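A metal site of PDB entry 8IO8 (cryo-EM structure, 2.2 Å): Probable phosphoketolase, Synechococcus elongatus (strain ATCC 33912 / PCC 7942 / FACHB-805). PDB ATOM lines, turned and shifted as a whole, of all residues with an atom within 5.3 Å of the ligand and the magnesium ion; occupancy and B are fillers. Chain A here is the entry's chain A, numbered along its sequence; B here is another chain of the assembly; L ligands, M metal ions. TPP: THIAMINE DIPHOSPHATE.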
ATOM      1  N   GLY A  62       7.248 -15.210 -10.086  1.00  0.00           N
ATOM      2  CA  GLY A  62       7.653 -14.795 -11.427  1.00  0.00           C
ATOM      3  C   GLY A  62       7.973 -13.318 -11.531  1.00  0.00           C
ATOM      4  O   GLY A  62       8.931 -12.933 -12.195  1.00  0.00           O
ATOM      5  N   SER A  63       7.187 -12.477 -10.868  1.00  0.00           N
ATOM      6  CA  SER A  63       7.388 -11.036 -10.979  1.00  0.00           C
ATOM      7  C   SER A  63       8.426 -10.490 -10.014  1.00  0.00           C
ATOM      8  O   SER A  63       8.880  -9.362 -10.201  1.00  0.00           O
ATOM      9  CB  SER A  63       6.058 -10.315 -10.773  1.00  0.00           C
ATOM     10  OG  SER A  63       6.124  -8.983 -11.227  1.00  0.00           O
ATOM     11  N   PRO A  91       2.099  -5.263 -10.255  1.00  0.00           N
ATOM     12  CA  PRO A  91       1.940  -6.667  -9.877  1.00  0.00           C
ATOM     13  C   PRO A  91       1.975  -6.851  -8.374  1.00  0.00           C
ATOM     14  O   PRO A  91       3.017  -7.165  -7.805  1.00  0.00           O
ATOM     15  CB  PRO A  91       3.143  -7.356 -10.549  1.00  0.00           C
ATOM     16  CG  PRO A  91       3.626  -6.395 -11.569  1.00  0.00           C
ATOM     17  CD  PRO A  91       3.346  -5.046 -11.004  1.00  0.00           C
ATOM     18  N   HIS A  93       0.975  -9.149  -6.564  1.00  0.00           N
ATOM     19  CA  HIS A  93       1.398 -10.475  -6.162  1.00  0.00           C
ATOM     20  C   HIS A  93       2.909 -10.575  -5.968  1.00  0.00           C
ATOM     21  O   HIS A  93       3.389 -11.561  -5.405  1.00  0.00           O
ATOM     22  CB  HIS A  93       0.924 -11.510  -7.177  1.00  0.00           C
ATOM     23  CG  HIS A  93       1.307 -11.181  -8.585  1.00  0.00           C
ATOM     24  ND1 HIS A  93       0.608 -10.288  -9.358  1.00  0.00           N
ATOM     25  CD2 HIS A  93       2.309 -11.642  -9.371  1.00  0.00           C
ATOM     26  CE1 HIS A  93       1.151 -10.200 -10.549  1.00  0.00           C
ATOM     27  NE2 HIS A  93       2.193 -11.018 -10.588  1.00  0.00           N
ATOM     28  N   GLY A 150      -1.894  -4.550  -5.685  1.00  0.00           N
ATOM     29  CA  GLY A 150      -2.174  -4.973  -7.040  1.00  0.00           C
ATOM     30  C   GLY A 150      -3.015  -6.228  -7.095  1.00  0.00           C
ATOM     31  O   GLY A 150      -2.779  -7.088  -7.946  1.00  0.00           O
ATOM     32  N   GLY A 151      -3.979  -6.351  -6.190  1.00  0.00           N
ATOM     33  CA  GLY A 151      -4.883  -7.479  -6.212  1.00  0.00           C
ATOM     34  C   GLY A 151      -5.789  -7.423  -7.421  1.00  0.00           C
ATOM     35  O   GLY A 151      -5.797  -8.335  -8.255  1.00  0.00           O
ATOM     36  N   GLU A 152      -6.563  -6.343  -7.520  1.00  0.00           N
ATOM     37  CA  GLU A 152      -7.353  -6.058  -8.708  1.00  0.00           C
ATOM     38  C   GLU A 152      -6.510  -5.211  -9.651  1.00  0.00           C
ATOM     39  O   GLU A 152      -6.154  -4.072  -9.321  1.00  0.00           O
ATOM     40  CB  GLU A 152      -8.651  -5.340  -8.324  1.00  0.00           C
ATOM     41  CG  GLU A 152      -9.546  -5.031  -9.499  1.00  0.00           C
ATOM     42  CD  GLU A 152     -10.210  -6.256 -10.053  1.00  0.00           C
ATOM     43  OE1 GLU A 152     -10.769  -7.039  -9.261  1.00  0.00           O
ATOM     44  OE2 GLU A 152     -10.171  -6.453 -11.284  1.00  0.00           O
ATOM     45  N   LEU A 153      -6.175  -5.762 -10.801  1.00  0.00           N
ATOM     46  CA  LEU A 153      -5.217  -5.126 -11.696  1.00  0.00           C
ATOM     47  C   LEU A 153      -5.882  -4.039 -12.537  1.00  0.00           C
ATOM     48  O   LEU A 153      -7.095  -4.072 -12.788  1.00  0.00           O
ATOM     49  CB  LEU A 153      -4.574  -6.172 -12.597  1.00  0.00           C
ATOM     50  CG  LEU A 153      -3.764  -7.227 -11.857  1.00  0.00           C
ATOM     51  CD1 LEU A 153      -3.333  -8.315 -12.814  1.00  0.00           C
ATOM     52  CD2 LEU A 153      -2.559  -6.614 -11.170  1.00  0.00           C
ATOM     53  N   GLY A 177       2.829  -4.481 -14.767  1.00  0.00           N
ATOM     54  CA  GLY A 177       2.928  -5.784 -15.382  1.00  0.00           C
ATOM     55  C   GLY A 177       2.301  -5.796 -16.766  1.00  0.00           C
ATOM     56  O   GLY A 177       1.296  -5.135 -17.022  1.00  0.00           O
ATOM     57  N   ASP A 178       2.919  -6.551 -17.671  1.00  0.00           N
ATOM     58  CA  ASP A 178       2.428  -6.574 -19.046  1.00  0.00           C
ATOM     59  C   ASP A 178       1.057  -7.233 -19.146  1.00  0.00           C
ATOM     60  O   ASP A 178       0.275  -6.902 -20.044  1.00  0.00           O
ATOM     61  CB  ASP A 178       3.432  -7.274 -19.956  1.00  0.00           C
ATOM     62  CG  ASP A 178       3.942  -8.570 -19.378  1.00  0.00           C
ATOM     63  OD1 ASP A 178       3.932  -8.727 -18.148  1.00  0.00           O
ATOM     64  OD2 ASP A 178       4.375  -9.437 -20.170  1.00  0.00           O
ATOM     65  N   GLY A 179       0.742  -8.175 -18.252  1.00  0.00           N
ATOM     66  CA  GLY A 179      -0.614  -8.673 -18.188  1.00  0.00           C
ATOM     67  C   GLY A 179      -1.592  -7.622 -17.711  1.00  0.00           C
ATOM     68  O   GLY A 179      -2.691  -7.491 -18.261  1.00  0.00           O
ATOM     69  N   GLU A 180      -1.204  -6.835 -16.712  1.00  0.00           N
ATOM     70  CA  GLU A 180      -2.053  -5.765 -16.205  1.00  0.00           C
ATOM     71  C   GLU A 180      -2.320  -4.712 -17.286  1.00  0.00           C
ATOM     72  O   GLU A 180      -3.385  -4.099 -17.302  1.00  0.00           O
ATOM     73  CB  GLU A 180      -1.412  -5.119 -14.984  1.00  0.00           C
ATOM     74  CG  GLU A 180      -2.217  -4.006 -14.356  1.00  0.00           C
ATOM     75  CD  GLU A 180      -1.442  -3.238 -13.315  1.00  0.00           C
ATOM     76  OE1 GLU A 180      -0.206  -3.438 -13.223  1.00  0.00           O
ATOM     77  OE2 GLU A 180      -2.059  -2.434 -12.573  1.00  0.00           O
ATOM     78  N   THR A 183      -5.587  -4.717 -19.325  1.00  0.00           N
ATOM     79  CA  THR A 183      -6.871  -4.395 -18.740  1.00  0.00           C
ATOM     80  C   THR A 183      -7.390  -3.058 -19.275  1.00  0.00           C
ATOM     81  O   THR A 183      -6.635  -2.220 -19.773  1.00  0.00           O
ATOM     82  CB  THR A 183      -6.792  -4.346 -17.214  1.00  0.00           C
ATOM     83  OG1 THR A 183      -5.915  -3.291 -16.820  1.00  0.00           O
ATOM     84  CG2 THR A 183      -6.263  -5.657 -16.674  1.00  0.00           C
ATOM     85  N   HIS A 209       6.894  -3.713 -16.981  1.00  0.00           N
ATOM     86  CA  HIS A 209       7.579  -4.960 -16.682  1.00  0.00           C
ATOM     87  C   HIS A 209       7.130  -5.997 -17.701  1.00  0.00           C
ATOM     88  O   HIS A 209       6.183  -6.748 -17.472  1.00  0.00           O
ATOM     89  CB  HIS A 209       7.307  -5.407 -15.261  1.00  0.00           C
ATOM     90  CG  HIS A 209       8.079  -6.627 -14.850  1.00  0.00           C
ATOM     91  ND1 HIS A 209       7.720  -7.410 -13.778  1.00  0.00           N
ATOM     92  CD2 HIS A 209       9.184  -7.190 -15.383  1.00  0.00           C
ATOM     93  CE1 HIS A 209       8.588  -8.398 -13.664  1.00  0.00           C
ATOM     94  NE2 HIS A 209       9.481  -8.295 -14.634  1.00  0.00           N
ATOM     95  N   ASN A 211       7.746  -9.032 -18.956  1.00  0.00           N
ATOM     96  CA  ASN A 211       8.364 -10.343 -18.819  1.00  0.00           C
ATOM     97  C   ASN A 211       7.785 -11.376 -19.793  1.00  0.00           C
ATOM     98  O   ASN A 211       8.257 -12.513 -19.800  1.00  0.00           O
ATOM     99  CB  ASN A 211       8.263 -10.862 -17.385  1.00  0.00           C
ATOM    100  CG  ASN A 211       6.858 -10.782 -16.825  1.00  0.00           C
ATOM    101  OD1 ASN A 211       5.891 -10.680 -17.568  1.00  0.00           O
ATOM    102  ND2 ASN A 211       6.746 -10.836 -15.513  1.00  0.00           N
ATOM    103  N   GLY A 212       6.778 -11.001 -20.576  1.00  0.00           N
ATOM    104  CA  GLY A 212       6.302 -11.826 -21.669  1.00  0.00           C
ATOM    105  C   GLY A 212       5.109 -12.691 -21.346  1.00  0.00           C
ATOM    106  O   GLY A 212       4.510 -13.236 -22.274  1.00  0.00           O
ATOM    107  N   TYR A 213       4.745 -12.835 -20.085  1.00  0.00           N
ATOM    108  CA  TYR A 213       3.671 -13.738 -19.698  1.00  0.00           C
ATOM    109  C   TYR A 213       2.908 -13.127 -18.524  1.00  0.00           C
ATOM    110  O   TYR A 213       3.416 -12.250 -17.826  1.00  0.00           O
ATOM    111  CB  TYR A 213       4.200 -15.130 -19.332  1.00  0.00           C
ATOM    112  CG  TYR A 213       4.946 -15.809 -20.444  1.00  0.00           C
ATOM    113  CD1 TYR A 213       4.276 -16.597 -21.372  1.00  0.00           C
ATOM    114  CD2 TYR A 213       6.322 -15.661 -20.584  1.00  0.00           C
ATOM    115  CE1 TYR A 213       4.959 -17.222 -22.392  1.00  0.00           C
ATOM    116  CE2 TYR A 213       7.006 -16.287 -21.605  1.00  0.00           C
ATOM    117  CZ  TYR A 213       6.310 -17.062 -22.508  1.00  0.00           C
ATOM    118  OH  TYR A 213       6.991 -17.688 -23.519  1.00  0.00           O
ATOM    119  N   LYS A 214       1.679 -13.603 -18.326  1.00  0.00           N
ATOM    120  CA  LYS A 214       0.885 -13.167 -17.186  1.00  0.00           C
ATOM    121  C   LYS A 214       0.599 -14.289 -16.194  1.00  0.00           C
ATOM    122  O   LYS A 214       1.069 -14.217 -15.052  1.00  0.00           O
ATOM    123  CB  LYS A 214      -0.430 -12.560 -17.697  1.00  0.00           C
ATOM    124  CG  LYS A 214      -0.867 -13.067 -19.055  1.00  0.00           C
ATOM    125  CD  LYS A 214      -2.147 -12.391 -19.518  1.00  0.00           C
ATOM    126  CE  LYS A 214      -2.561 -12.888 -20.889  1.00  0.00           C
ATOM    127  NZ  LYS A 214      -3.774 -12.187 -21.382  1.00  0.00           N
ATOM    128  N   ILE A 215      -0.127 -15.328 -16.584  1.00  0.00           N
ATOM    129  CA  ILE A 215      -0.322 -16.483 -15.724  1.00  0.00           C
ATOM    130  C   ILE A 215      -0.003 -17.758 -16.490  1.00  0.00           C
ATOM    131  O   ILE A 215       0.835 -18.566 -16.066  1.00  0.00           O
ATOM    132  CB  ILE A 215      -1.753 -16.541 -15.153  1.00  0.00           C
ATOM    133  CG1 ILE A 215      -1.934 -15.470 -14.079  1.00  0.00           C
ATOM    134  CG2 ILE A 215      -2.039 -17.913 -14.569  1.00  0.00           C
ATOM    135  CD1 ILE A 215      -3.156 -15.683 -13.207  1.00  0.00           C
ATOM    136  N   THR A 219       1.626 -12.347 -22.959  1.00  0.00           N
ATOM    137  CA  THR A 219       0.928 -11.074 -22.977  1.00  0.00           C
ATOM    138  C   THR A 219       0.967 -10.482 -24.382  1.00  0.00           C
ATOM    139  O   THR A 219       1.952 -10.646 -25.106  1.00  0.00           O
ATOM    140  CB  THR A 219       1.556 -10.096 -21.983  1.00  0.00           C
ATOM    141  OG1 THR A 219       2.944  -9.938 -22.276  1.00  0.00           O
ATOM    142  CG2 THR A 219       1.408 -10.645 -20.576  1.00  0.00           C
ATOM    143  N   LYS A 293      10.735 -14.074 -17.093  1.00  0.00           N
ATOM    144  CA  LYS A 293       9.890 -14.260 -15.927  1.00  0.00           C
ATOM    145  C   LYS A 293      10.452 -15.386 -15.068  1.00  0.00           C
ATOM    146  O   LYS A 293      10.837 -16.445 -15.587  1.00  0.00           O
ATOM    147  CB  LYS A 293       8.458 -14.566 -16.341  1.00  0.00           C
ATOM    148  CG  LYS A 293       7.473 -14.559 -15.191  1.00  0.00           C
ATOM    149  CD  LYS A 293       6.044 -14.555 -15.682  1.00  0.00           C
ATOM    150  CE  LYS A 293       5.068 -14.374 -14.535  1.00  0.00           C
ATOM    151  NZ  LYS A 293       3.675 -14.226 -15.003  1.00  0.00           N
ATOM    152  N   HIS A 313       5.176 -18.268 -12.695  1.00  0.00           N
ATOM    153  CA  HIS A 313       4.332 -17.185 -12.186  1.00  0.00           C
ATOM    154  C   HIS A 313       4.040 -17.358 -10.697  1.00  0.00           C
ATOM    155  O   HIS A 313       4.262 -16.439  -9.903  1.00  0.00           O
ATOM    156  CB  HIS A 313       3.035 -17.118 -12.979  1.00  0.00           C
ATOM    157  CG  HIS A 313       2.006 -16.222 -12.363  1.00  0.00           C
ATOM    158  ND1 HIS A 313       2.064 -14.849 -12.471  1.00  0.00           N
ATOM    159  CD2 HIS A 313       0.902 -16.502 -11.629  1.00  0.00           C
ATOM    160  CE1 HIS A 313       1.026 -14.321 -11.826  1.00  0.00           C
ATOM    161  NE2 HIS A 313       0.314 -15.303 -11.316  1.00  0.00           N
ATOM    162  N   PRO B 425     -10.554 -15.167 -18.778  1.00  0.00           N
ATOM    163  CA  PRO B 425      -9.454 -14.204 -18.607  1.00  0.00           C
ATOM    164  C   PRO B 425      -8.170 -14.833 -18.076  1.00  0.00           C
ATOM    165  O   PRO B 425      -7.746 -14.618 -16.935  1.00  0.00           O
ATOM    166  CB  PRO B 425     -10.055 -13.193 -17.623  1.00  0.00           C
ATOM    167  CG  PRO B 425     -11.125 -13.963 -16.867  1.00  0.00           C
ATOM    168  CD  PRO B 425     -11.359 -15.281 -17.552  1.00  0.00           C
ATOM    169  N   ASP B 426      -7.535 -15.644 -18.928  1.00  0.00           N
ATOM    170  CA  ASP B 426      -6.306 -16.344 -18.587  1.00  0.00           C
ATOM    171  C   ASP B 426      -6.473 -17.173 -17.324  1.00  0.00           C
ATOM    172  O   ASP B 426      -5.588 -17.250 -16.468  1.00  0.00           O
ATOM    173  CB  ASP B 426      -5.134 -15.364 -18.446  1.00  0.00           C
ATOM    174  CG  ASP B 426      -3.788 -16.062 -18.457  1.00  0.00           C
ATOM    175  OD1 ASP B 426      -3.736 -17.256 -18.794  1.00  0.00           O
ATOM    176  OD2 ASP B 426      -2.783 -15.408 -18.100  1.00  0.00           O
ATOM    177  N   GLU B 427      -7.644 -17.811 -17.206  1.00  0.00           N
ATOM    178  CA  GLU B 427      -7.948 -18.634 -16.047  1.00  0.00           C
ATOM    179  C   GLU B 427      -8.452 -20.015 -16.420  1.00  0.00           C
ATOM    180  O   GLU B 427      -8.842 -20.772 -15.522  1.00  0.00           O
ATOM    181  CB  GLU B 427      -8.974 -17.931 -15.143  1.00  0.00           C
ATOM    182  CG  GLU B 427      -8.438 -16.668 -14.488  1.00  0.00           C
ATOM    183  CD  GLU B 427      -9.523 -15.867 -13.793  1.00  0.00           C
ATOM    184  OE1 GLU B 427     -10.709 -16.229 -13.928  1.00  0.00           O
ATOM    185  OE2 GLU B 427      -9.189 -14.875 -13.116  1.00  0.00           O
ATOM    186  N   LEU B 468      -6.817 -10.739 -20.811  1.00  0.00           N
ATOM    187  CA  LEU B 468      -6.939 -10.407 -19.395  1.00  0.00           C
ATOM    188  C   LEU B 468      -7.989  -9.348 -19.118  1.00  0.00           C
ATOM    189  O   LEU B 468      -8.267  -9.064 -17.952  1.00  0.00           O
ATOM    190  CB  LEU B 468      -5.595  -9.938 -18.847  1.00  0.00           C
ATOM    191  CG  LEU B 468      -5.379 -10.407 -17.408  1.00  0.00           C
ATOM    192  CD1 LEU B 468      -5.584 -11.904 -17.355  1.00  0.00           C
ATOM    193  CD2 LEU B 468      -4.012 -10.026 -16.892  1.00  0.00           C
ATOM    194  N   GLU B 470     -11.565  -8.305 -18.626  1.00  0.00           N
ATOM    195  CA  GLU B 470     -12.919  -8.819 -18.447  1.00  0.00           C
ATOM    196  C   GLU B 470     -13.938  -8.031 -19.252  1.00  0.00           C
ATOM    197  O   GLU B 470     -14.932  -8.597 -19.714  1.00  0.00           O
ATOM    198  CB  GLU B 470     -13.297  -8.800 -16.967  1.00  0.00           C
ATOM    199  CG  GLU B 470     -12.720  -9.933 -16.146  1.00  0.00           C
ATOM    200  CD  GLU B 470     -11.258  -9.736 -15.826  1.00  0.00           C
ATOM    201  OE1 GLU B 470     -10.723  -8.644 -16.108  1.00  0.00           O
ATOM    202  OE2 GLU B 470     -10.633 -10.677 -15.279  1.00  0.00           O
ATOM    203  N   PHE B 495     -13.238 -11.397  -9.418  1.00  0.00           N
ATOM    204  CA  PHE B 495     -13.181 -10.389 -10.467  1.00  0.00           C
ATOM    205  C   PHE B 495     -14.504 -10.244 -11.208  1.00  0.00           C
ATOM    206  O   PHE B 495     -14.518  -9.771 -12.346  1.00  0.00           O
ATOM    207  CB  PHE B 495     -12.052 -10.709 -11.433  1.00  0.00           C
ATOM    208  CG  PHE B 495     -10.764 -11.062 -10.742  1.00  0.00           C
ATOM    209  CD1 PHE B 495     -10.079 -10.114 -10.016  1.00  0.00           C
ATOM    210  CD2 PHE B 495     -10.270 -12.353 -10.797  1.00  0.00           C
ATOM    211  CE1 PHE B 495      -8.902 -10.437  -9.365  1.00  0.00           C
ATOM    212  CE2 PHE B 495      -9.089 -12.686 -10.146  1.00  0.00           C
ATOM    213  CZ  PHE B 495      -8.418 -11.722  -9.433  1.00  0.00           C
ATOM    214  N   VAL B 498     -16.028  -6.544 -11.887  1.00  0.00           N
ATOM    215  CA  VAL B 498     -15.524  -5.771 -13.011  1.00  0.00           C
ATOM    216  C   VAL B 498     -16.590  -5.644 -14.095  1.00  0.00           C
ATOM    217  O   VAL B 498     -16.684  -4.607 -14.758  1.00  0.00           O
ATOM    218  CB  VAL B 498     -14.244  -6.426 -13.551  1.00  0.00           C
ATOM    219  CG1 VAL B 498     -13.676  -5.618 -14.706  1.00  0.00           C
ATOM    220  CG2 VAL B 498     -13.221  -6.547 -12.448  1.00  0.00           C
ATOM    221  N   ASN B 540      -4.165 -16.941  -6.441  1.00  0.00           N
ATOM    222  CA  ASN B 540      -4.605 -15.717  -7.108  1.00  0.00           C
ATOM    223  C   ASN B 540      -5.894 -15.192  -6.487  1.00  0.00           C
ATOM    224  O   ASN B 540      -6.704 -15.965  -5.968  1.00  0.00           O
ATOM    225  CB  ASN B 540      -4.815 -15.978  -8.597  1.00  0.00           C
ATOM    226  CG  ASN B 540      -6.091 -16.735  -8.898  1.00  0.00           C
ATOM    227  OD1 ASN B 540      -6.190 -17.936  -8.641  1.00  0.00           O
ATOM    228  ND2 ASN B 540      -7.078 -16.032  -9.428  1.00  0.00           N
ATOM    229  N   GLY B 541      -6.079 -13.880  -6.536  1.00  0.00           N
ATOM    230  CA  GLY B 541      -7.265 -13.273  -5.982  1.00  0.00           C
ATOM    231  C   GLY B 541      -6.941 -12.482  -4.728  1.00  0.00           C
ATOM    232  O   GLY B 541      -6.155 -12.941  -3.892  1.00  0.00           O
HETATM  233  N1' TPP L   1      -8.132 -10.185 -13.795  1.00  0.00           N
HETATM  234  C2' TPP L   1      -7.954  -8.999 -13.191  1.00  0.00           C
HETATM  235  CM2 TPP L   1      -8.718  -7.834 -13.730  1.00  0.00           C
HETATM  236  N3' TPP L   1      -7.152  -8.769 -12.155  1.00  0.00           N
HETATM  237  C4' TPP L   1      -6.466  -9.816 -11.661  1.00  0.00           C
HETATM  238  N4' TPP L   1      -5.665  -9.564 -10.614  1.00  0.00           N
HETATM  239  C5' TPP L   1      -6.587 -11.118 -12.227  1.00  0.00           C
HETATM  240  C6' TPP L   1      -7.445 -11.210 -13.299  1.00  0.00           C
HETATM  241  C7' TPP L   1      -5.837 -12.312 -11.715  1.00  0.00           C
HETATM  242  N3  TPP L   1      -4.364 -12.109 -11.675  1.00  0.00           N
HETATM  243  C2  TPP L   1      -3.696 -11.886 -10.565  1.00  0.00           C
HETATM  244  S1  TPP L   1      -2.049 -11.701 -10.851  1.00  0.00           S
HETATM  245  C5  TPP L   1      -2.278 -11.943 -12.543  1.00  0.00           C
HETATM  246  C4  TPP L   1      -3.578 -12.151 -12.825  1.00  0.00           C
HETATM  247  CM4 TPP L   1      -4.186 -12.400 -14.150  1.00  0.00           C
HETATM  248  C6  TPP L   1      -1.115 -11.906 -13.500  1.00  0.00           C
HETATM  249  C7  TPP L   1      -1.037 -10.612 -14.279  1.00  0.00           C
HETATM  250  O7  TPP L   1       0.129 -10.666 -15.138  1.00  0.00           O
HETATM  251  PA  TPP L   1       1.246  -9.564 -15.181  1.00  0.00           P
HETATM  252  O1A TPP L   1       1.999  -9.731 -16.488  1.00  0.00           O
HETATM  253  O2A TPP L   1       0.661  -8.237 -14.929  1.00  0.00           O
HETATM  254  O3A TPP L   1       2.222 -10.003 -14.024  1.00  0.00           O
HETATM  255  PB  TPP L   1       3.690 -10.560 -13.829  1.00  0.00           P
HETATM  256  O1B TPP L   1       3.563 -11.539 -12.673  1.00  0.00           O
HETATM  257  O2B TPP L   1       3.979 -11.338 -15.107  1.00  0.00           O
HETATM  258  O3B TPP L   1       4.661  -9.451 -13.580  1.00  0.00           O
HETATM  259 MG    MG M   1       3.891 -10.413 -16.972  1.00  0.00          MG
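N of Asp 178 is in hydrogen-bond range of O of His 209 (3.3 Å).
The side-chain hydroxyl (OG1) of Thr 219 sits at hydrogen-bond distance from the side-chain carboxylate (OD2) of Asp 178, at 2.6 Å.
The side-chain hydroxyl (OG) of Ser 63 lies within hydrogen-bond range of a ring nitrogen (ND1) of His 209 (3.4 Å).
The side-chain amino group (NZ) of Lys 293 is in hydrogen-bond range of a ring nitrogen (ND1) of His 313 (3.1 Å).
The side-chain hydroxyl (OG1) of Thr 183 is in hydrogen-bond range of the backbone carbonyl oxygen (O) of Glu 180 (2.7 Å).
O of Lys 214 sits at hydrogen-bond distance from ND1 of His 313 (2.8 Å).
The side-chain carboxylate (OD2) of Asp 426 of chain B is in hydrogen-bond range of the backbone NH (N) of Ile 215.
The backbone NH (N) of Gly 62 sits at hydrogen-bond distance from the backbone carbonyl oxygen (O) of His 313 (3.2 Å).
NE2 of His 93 is in hydrogen-bond range of O1B of the ligand.
The backbone carbonyl oxygen (O) of Gly 151 is in hydrogen-bond range of a nitrogen (N4') of the ligand.
An oxygen (O2A) of the ligand lies within hydrogen-bond range of the backbone NH of Gly 179, 3.3 Å away.
The side-chain hydroxyl (OG) of Ser 63 is in hydrogen-bond range of an oxygen (O3B) of the ligand.
The side-chain amino group (NZ) of Lys 293 lies within salt-bridge range of an oxygen (O1B) of the ligand (3.6 Å).
An oxygen (O2A) of the ligand is in hydrogen-bond range of the backbone NH (N) of Glu 180 (2.9 Å).
The backbone NH (N) of Leu 153 is in hydrogen-bond range of a nitrogen (N3') of the ligand.
The magnesium ion is bound by the side-chain carboxylate (OD1) of Asp 178 (2.1 Å), an oxygen (O1A) of the ligand (2.1 Å), the backbone carbonyl oxygen (O) of Tyr 213 (2.1 Å), an oxygen (O2B) of the ligand (2.1 Å) and the side-chain amide oxygen (OD1) of Asn 211 (2.1 Å).
Of the 31 residues printed, 3 come within 4 Å of the magnesium ion.
The nearest printed residue that does not touch the magnesium ion is Gly 179 (4.1 Å).
OE2 of Glu 470 of chain B sits close to N1' of the ligand, 2.9 Å away.
Merely in contact with the ligand: Pro 91 (3.8 Å), Glu 152 (3.2 Å), Gly 177 (3.4 Å), His 209 (3.7 Å), Lys 214 (3.2 Å), Ile 215 (3.6 Å), His 313 (3.6 Å), Leu 468 of chain B (3.5 Å) and Phe 495 of chain B (3.4 Å).
Hydrophobic or aromatic side chains that line the ligand: Pro 91, His 93, Leu 153, Ile 215, His 313, Leu 468 of chain B and Phe 495 of chain B.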
